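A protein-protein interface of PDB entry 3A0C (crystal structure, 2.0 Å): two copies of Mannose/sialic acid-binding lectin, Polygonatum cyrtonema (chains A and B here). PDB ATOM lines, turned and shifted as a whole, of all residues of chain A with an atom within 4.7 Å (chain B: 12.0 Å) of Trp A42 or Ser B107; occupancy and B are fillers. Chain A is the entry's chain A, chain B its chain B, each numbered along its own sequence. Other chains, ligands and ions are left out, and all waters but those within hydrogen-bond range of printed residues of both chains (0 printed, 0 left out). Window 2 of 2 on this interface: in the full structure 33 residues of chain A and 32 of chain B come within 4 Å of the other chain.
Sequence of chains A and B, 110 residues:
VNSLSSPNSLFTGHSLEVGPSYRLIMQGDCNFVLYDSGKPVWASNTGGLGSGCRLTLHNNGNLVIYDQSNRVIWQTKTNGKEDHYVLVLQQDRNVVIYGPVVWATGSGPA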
ATOM      1  N   PHE A  32     -14.266 -11.067  15.059  1.00  0.00           N
ATOM      2  CA  PHE A  32     -15.105 -11.621  14.002  1.00  0.00           C
ATOM      3  C   PHE A  32     -16.448 -11.939  14.647  1.00  0.00           C
ATOM      4  O   PHE A  32     -16.576 -12.910  15.400  1.00  0.00           O
ATOM      5  CB  PHE A  32     -14.462 -12.883  13.419  1.00  0.00           C
ATOM      6  CG  PHE A  32     -15.193 -13.439  12.239  1.00  0.00           C
ATOM      7  CD1 PHE A  32     -15.510 -12.622  11.162  1.00  0.00           C
ATOM      8  CD2 PHE A  32     -15.565 -14.780  12.202  1.00  0.00           C
ATOM      9  CE1 PHE A  32     -16.188 -13.125  10.062  1.00  0.00           C
ATOM     10  CE2 PHE A  32     -16.250 -15.300  11.097  1.00  0.00           C
ATOM     11  CZ  PHE A  32     -16.560 -14.469  10.028  1.00  0.00           C
ATOM     12  N   VAL A  33     -17.452 -11.115  14.349  1.00  0.00           N
ATOM     13  CA  VAL A  33     -18.767 -11.276  14.948  1.00  0.00           C
ATOM     14  C   VAL A  33     -19.979 -11.343  14.009  1.00  0.00           C
ATOM     15  O   VAL A  33     -20.011 -10.729  12.937  1.00  0.00           O
ATOM     16  CB  VAL A  33     -18.978 -10.159  16.023  1.00  0.00           C
ATOM     17  CG1 VAL A  33     -18.161  -8.939  15.672  1.00  0.00           C
ATOM     18  CG2 VAL A  33     -20.438  -9.795  16.133  1.00  0.00           C
ATOM     19  N   LEU A  34     -20.978 -12.106  14.438  1.00  0.00           N
ATOM     20  CA  LEU A  34     -22.219 -12.290  13.691  1.00  0.00           C
ATOM     21  C   LEU A  34     -23.301 -11.391  14.271  1.00  0.00           C
ATOM     22  O   LEU A  34     -23.603 -11.481  15.454  1.00  0.00           O
ATOM     23  CB  LEU A  34     -22.667 -13.754  13.783  1.00  0.00           C
ATOM     24  CG  LEU A  34     -24.038 -14.128  13.229  1.00  0.00           C
ATOM     25  CD1 LEU A  34     -24.159 -13.733  11.772  1.00  0.00           C
ATOM     26  CD2 LEU A  34     -24.223 -15.618  13.383  1.00  0.00           C
ATOM     27  N   PRO A  40     -25.273  -8.573  18.522  1.00  0.00           N
ATOM     28  CA  PRO A  40     -24.236  -9.587  18.324  1.00  0.00           C
ATOM     29  C   PRO A  40     -24.694 -10.923  18.927  1.00  0.00           C
ATOM     30  O   PRO A  40     -24.877 -11.032  20.142  1.00  0.00           O
ATOM     31  CB  PRO A  40     -23.027  -8.991  19.043  1.00  0.00           C
ATOM     32  CG  PRO A  40     -23.640  -8.145  20.107  1.00  0.00           C
ATOM     33  CD  PRO A  40     -24.794  -7.492  19.402  1.00  0.00           C
ATOM     34  N   VAL A  41     -24.898 -11.926  18.068  1.00  0.00           N
ATOM     35  CA  VAL A  41     -25.343 -13.255  18.503  1.00  0.00           C
ATOM     36  C   VAL A  41     -24.180 -14.237  18.551  1.00  0.00           C
ATOM     37  O   VAL A  41     -24.306 -15.323  19.114  1.00  0.00           O
ATOM     38  CB  VAL A  41     -26.417 -13.841  17.557  1.00  0.00           C
ATOM     39  CG1 VAL A  41     -27.550 -12.856  17.389  1.00  0.00           C
ATOM     40  CG2 VAL A  41     -25.793 -14.193  16.205  1.00  0.00           C
ATOM     41  N   TRP A  42     -23.054 -13.865  17.948  1.00  0.00           N
ATOM     42  CA  TRP A  42     -21.871 -14.726  17.941  1.00  0.00           C
ATOM     43  C   TRP A  42     -20.601 -13.926  17.641  1.00  0.00           C
ATOM     44  O   TRP A  42     -20.653 -12.918  16.935  1.00  0.00           O
ATOM     45  CB  TRP A  42     -22.018 -15.847  16.899  1.00  0.00           C
ATOM     46  CG  TRP A  42     -20.895 -16.844  16.972  1.00  0.00           C
ATOM     47  CD1 TRP A  42     -20.860 -17.996  17.711  1.00  0.00           C
ATOM     48  CD2 TRP A  42     -19.612 -16.736  16.334  1.00  0.00           C
ATOM     49  NE1 TRP A  42     -19.633 -18.611  17.574  1.00  0.00           N
ATOM     50  CE2 TRP A  42     -18.850 -17.859  16.736  1.00  0.00           C
ATOM     51  CE3 TRP A  42     -19.037 -15.801  15.463  1.00  0.00           C
ATOM     52  CZ2 TRP A  42     -17.537 -18.070  16.296  1.00  0.00           C
ATOM     53  CZ3 TRP A  42     -17.730 -16.009  15.024  1.00  0.00           C
ATOM     54  CH2 TRP A  42     -16.994 -17.139  15.445  1.00  0.00           C
ATOM     55  N   ALA A  43     -19.465 -14.382  18.170  1.00  0.00           N
ATOM     56  CA  ALA A  43     -18.195 -13.698  17.939  1.00  0.00           C
ATOM     57  C   ALA A  43     -17.000 -14.575  18.273  1.00  0.00           C
ATOM     58  O   ALA A  43     -17.111 -15.505  19.080  1.00  0.00           O
ATOM     59  CB  ALA A  43     -18.142 -12.412  18.760  1.00  0.00           C
ATOM     60  N   SER A  44     -15.868 -14.292  17.631  1.00  0.00           N
ATOM     61  CA  SER A  44     -14.635 -15.033  17.879  1.00  0.00           C
ATOM     62  C   SER A  44     -14.005 -14.510  19.174  1.00  0.00           C
ATOM     63  O   SER A  44     -13.054 -15.088  19.684  1.00  0.00           O
ATOM     64  CB  SER A  44     -13.656 -14.859  16.722  1.00  0.00           C
ATOM     65  OG  SER A  44     -13.339 -13.494  16.552  1.00  0.00           O
ATOM     66  N   TRP A  74      -6.691 -16.336  15.748  1.00  0.00           N
ATOM     67  CA  TRP A  74      -7.803 -17.256  15.995  1.00  0.00           C
ATOM     68  C   TRP A  74      -7.889 -18.251  14.831  1.00  0.00           C
ATOM     69  O   TRP A  74      -7.521 -17.925  13.704  1.00  0.00           O
ATOM     70  CB  TRP A  74      -9.098 -16.436  16.089  1.00  0.00           C
ATOM     71  CG  TRP A  74     -10.375 -17.188  16.319  1.00  0.00           C
ATOM     72  CD1 TRP A  74     -10.972 -17.430  17.517  1.00  0.00           C
ATOM     73  CD2 TRP A  74     -11.244 -17.748  15.317  1.00  0.00           C
ATOM     74  NE1 TRP A  74     -12.159 -18.099  17.330  1.00  0.00           N
ATOM     75  CE2 TRP A  74     -12.349 -18.307  15.989  1.00  0.00           C
ATOM     76  CE3 TRP A  74     -11.191 -17.828  13.917  1.00  0.00           C
ATOM     77  CZ2 TRP A  74     -13.395 -18.942  15.311  1.00  0.00           C
ATOM     78  CZ3 TRP A  74     -12.227 -18.455  13.247  1.00  0.00           C
ATOM     79  CH2 TRP A  74     -13.315 -19.004  13.944  1.00  0.00           C
ATOM     80  N   ARG A  93     -29.411 -18.512  10.123  1.00  0.00           N
ATOM     81  CA  ARG A  93     -28.445 -17.809  10.951  1.00  0.00           C
ATOM     82  C   ARG A  93     -27.217 -18.596  11.401  1.00  0.00           C
ATOM     83  O   ARG A  93     -26.380 -18.064  12.135  1.00  0.00           O
ATOM     84  CB  ARG A  93     -29.139 -17.193  12.175  1.00  0.00           C
ATOM     85  CG  ARG A  93     -28.534 -15.836  12.575  1.00  0.00           C
ATOM     86  CD  ARG A  93     -29.148 -15.271  13.847  1.00  0.00           C
ATOM     87  NE  ARG A  93     -28.927 -16.158  14.983  1.00  0.00           N
ATOM     88  CZ  ARG A  93     -29.363 -15.926  16.218  1.00  0.00           C
ATOM     89  NH1 ARG A  93     -30.047 -14.831  16.506  1.00  0.00           N
ATOM     90  NH2 ARG A  93     -29.125 -16.806  17.166  1.00  0.00           N
ATOM     91  N   ASN A  94     -27.088 -19.845  10.975  1.00  0.00           N
ATOM     92  CA  ASN A  94     -25.922 -20.637  11.358  1.00  0.00           C
ATOM     93  C   ASN A  94     -24.840 -20.350  10.321  1.00  0.00           C
ATOM     94  O   ASN A  94     -25.143 -20.154   9.161  1.00  0.00           O
ATOM     95  CB  ASN A  94     -26.273 -22.140  11.378  1.00  0.00           C
ATOM     96  CG  ASN A  94     -25.235 -23.003  12.122  1.00  0.00           C
ATOM     97  OD1 ASN A  94     -24.298 -22.512  12.740  1.00  0.00           O
ATOM     98  ND2 ASN A  94     -25.425 -24.307  12.062  1.00  0.00           N
ATOM     99  N   VAL A  95     -23.587 -20.288  10.759  1.00  0.00           N
ATOM    100  CA  VAL A  95     -22.448 -20.042   9.877  1.00  0.00           C
ATOM    101  C   VAL A  95     -21.654 -21.336   9.802  1.00  0.00           C
ATOM    102  O   VAL A  95     -21.030 -21.757  10.777  1.00  0.00           O
ATOM    103  CB  VAL A  95     -21.557 -18.920  10.425  1.00  0.00           C
ATOM    104  CG1 VAL A  95     -20.293 -18.806   9.589  1.00  0.00           C
ATOM    105  CG2 VAL A  95     -22.343 -17.599  10.421  1.00  0.00           C
ATOM    106  N   TRP B 103     -17.139 -27.388  10.061  1.00  0.00           N
ATOM    107  CA  TRP B 103     -17.211 -26.551  11.248  1.00  0.00           C
ATOM    108  C   TRP B 103     -18.432 -25.641  11.131  1.00  0.00           C
ATOM    109  O   TRP B 103     -18.953 -25.440  10.036  1.00  0.00           O
ATOM    110  CB  TRP B 103     -15.930 -25.714  11.347  1.00  0.00           C
ATOM    111  CG  TRP B 103     -15.819 -24.834  12.582  1.00  0.00           C
ATOM    112  CD1 TRP B 103     -15.350 -25.189  13.817  1.00  0.00           C
ATOM    113  CD2 TRP B 103     -16.154 -23.449  12.666  1.00  0.00           C
ATOM    114  NE1 TRP B 103     -15.366 -24.108  14.658  1.00  0.00           N
ATOM    115  CE2 TRP B 103     -15.853 -23.022  13.978  1.00  0.00           C
ATOM    116  CE3 TRP B 103     -16.674 -22.520  11.755  1.00  0.00           C
ATOM    117  CZ2 TRP B 103     -16.052 -21.701  14.402  1.00  0.00           C
ATOM    118  CZ3 TRP B 103     -16.869 -21.214  12.176  1.00  0.00           C
ATOM    119  CH2 TRP B 103     -16.557 -20.818  13.487  1.00  0.00           C
ATOM    120  N   ALA B 104     -18.901 -25.116  12.264  1.00  0.00           N
ATOM    121  CA  ALA B 104     -20.048 -24.219  12.292  1.00  0.00           C
ATOM    122  C   ALA B 104     -19.927 -23.393  13.551  1.00  0.00           C
ATOM    123  O   ALA B 104     -19.258 -23.816  14.489  1.00  0.00           O
ATOM    124  CB  ALA B 104     -21.343 -25.012  12.322  1.00  0.00           C
ATOM    125  N   THR B 105     -20.573 -22.225  13.582  1.00  0.00           N
ATOM    126  CA  THR B 105     -20.509 -21.361  14.764  1.00  0.00           C
ATOM    127  C   THR B 105     -21.529 -21.788  15.821  1.00  0.00           C
ATOM    128  O   THR B 105     -21.322 -21.582  17.020  1.00  0.00           O
ATOM    129  CB  THR B 105     -20.776 -19.873  14.411  1.00  0.00           C
ATOM    130  OG1 THR B 105     -21.984 -19.774  13.647  1.00  0.00           O
ATOM    131  CG2 THR B 105     -19.613 -19.281  13.617  1.00  0.00           C
ATOM    132  N   GLY B 106     -22.612 -22.415  15.370  1.00  0.00           N
ATOM    133  CA  GLY B 106     -23.661 -22.820  16.288  1.00  0.00           C
ATOM    134  C   GLY B 106     -24.578 -21.638  16.590  1.00  0.00           C
ATOM    135  O   GLY B 106     -25.394 -21.686  17.510  1.00  0.00           O
ATOM    136  N   SER B 107     -24.437 -20.564  15.818  1.00  0.00           N
ATOM    137  CA  SER B 107     -25.259 -19.371  15.994  1.00  0.00           C
ATOM    138  C   SER B 107     -26.640 -19.625  15.403  1.00  0.00           C
ATOM    139  O   SER B 107     -27.571 -18.844  15.554  1.00  0.00           O
ATOM    140  CB  SER B 107     -24.608 -18.177  15.310  1.00  0.00           C
ATOM    141  OG  SER B 107     -24.269 -18.485  13.970  1.00  0.00           O
ATOM    142  N   GLY B 108     -26.772 -20.750  14.728  1.00  0.00           N
ATOM    143  CA  GLY B 108     -28.045 -21.116  14.145  1.00  0.00           C
ATOM    144  C   GLY B 108     -28.214 -22.600  14.388  1.00  0.00           C
ATOM    145  O   GLY B 108     -27.326 -23.209  14.967  1.00  0.00           O
ATOM    146  N   PRO B 109     -29.322 -23.220  13.970  1.00  0.00           N
ATOM    147  CA  PRO B 109     -30.457 -22.623  13.272  1.00  0.00           C
ATOM    148  C   PRO B 109     -31.319 -21.761  14.183  1.00  0.00           C
ATOM    149  O   PRO B 109     -31.095 -21.777  15.410  1.00  0.00           O
ATOM    150  CB  PRO B 109     -31.212 -23.842  12.756  1.00  0.00           C
ATOM    151  CG  PRO B 109     -30.996 -24.822  13.832  1.00  0.00           C
ATOM    152  CD  PRO B 109     -29.520 -24.670  14.122  1.00  0.00           C
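Among the printed residues, merely in contact across the chains: Leu A34 with Ser B107, Trp A42 with Ser B107, Trp A74 with Trp B103, Arg A93 with Gly B108, Asn A94 with Ala B104, Asn A94 with Thr B105, Asn A94 with Ser B107, Asn A94 with Gly B108, Val A95 with Ala B104 and Val A95 with Ser B107.
No residue of chain B comes within 4 Å of Phe A32.
Leu A34 touches just one residue of chain B: Ser B107.
No residue of chain B comes within 4 Å of Pro A40.
Of chain B, only Thr B105 and Ser B107 come within 4 Å of Trp A42.
No residue of chain B comes within 4 Å of Ser A44.
Arg A93 touches two residues of chain B.
Asn A94 touches just these residues of chain B: Ala B104, Thr B105, Gly B106, Ser B107 and Gly B108.
Val A95 touches just these residues of chain B: Ala B104 (3.1 Å), Thr B105 (2.9 Å) and Ser B107 (3.7 Å).
Of the printed residues of chain A, Trp B103 touches Trp A74 (3.7 Å).
Printed residues of chain A within 4 Å of Ala B104: Asn A94 and Val A95.
Printed residues of chain A within 4 Å of Thr B105: Trp A42 (3.5 Å), Asn A94 (3.7 Å) and Val A95 (2.9 Å).
Of the printed residues of chain A, Gly B106 touches Asn A94.
Ser B107 touches just these residues of chain A: Leu A34, Trp A42, Arg A93, Asn A94 and Val A95.
Of the printed residues of chain A, Gly B108 touches Arg A93 (3.8 Å) and Asn A94 (3.4 Å).
The nearest printed residue of chain A that does not touch Ala B104 is Trp A42 (6.1 Å).
Of the 12 printed residues of chain A, 6 touch a printed residue of chain B.
Hydrophobic or aromatic side chains of chain A that line the printed part of chain B: Leu A34, Trp A42, Trp A74 and Val A95.
Of the 7 printed residues of chain B, 6 touch a printed residue of chain A.
Hydrophobic or aromatic side chains of chain B that line the printed part of chain A: Trp B103 and Ala B104.
Along chain B the printed residues that touch a printed residue of chain A span positions 103 to 108.
No position is printed for both chains.
Of the 14 pairs that touch across the chains among the printed residues, none has its exchanged pair printed and touching as well.
The backbone carbonyl oxygen (O) of Leu A34 lies within hydrogen-bond range of the backbone NH (N) of Val A41 (3.0 Å).
The backbone carbonyl oxygen (O) of Trp A42 lies within hydrogen-bond range of the backbone NH (N) of Leu A34, 2.6 Å away.
The side-chain hydroxyl (OG1) of Thr B105 lies within hydrogen-bond range of the side-chain hydroxyl (OG) of Ser B107, 2.6 Å away.
The indole nitrogen (NE1) of Trp A42 sits at hydrogen-bond distance from the backbone carbonyl oxygen (O) of Thr B105, at 3.5 Å.
The backbone carbonyl oxygen of Arg A93 sits at hydrogen-bond distance from the side-chain hydroxyl of Ser B107 (2.8 Å).
The backbone NH of Gly B106 sits at hydrogen-bond distance from the side-chain amide oxygen of Asn A94.
The backbone NH (N) of Thr B105 lies within hydrogen-bond range of the backbone carbonyl oxygen (O) of Val A95 (2.9 Å).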
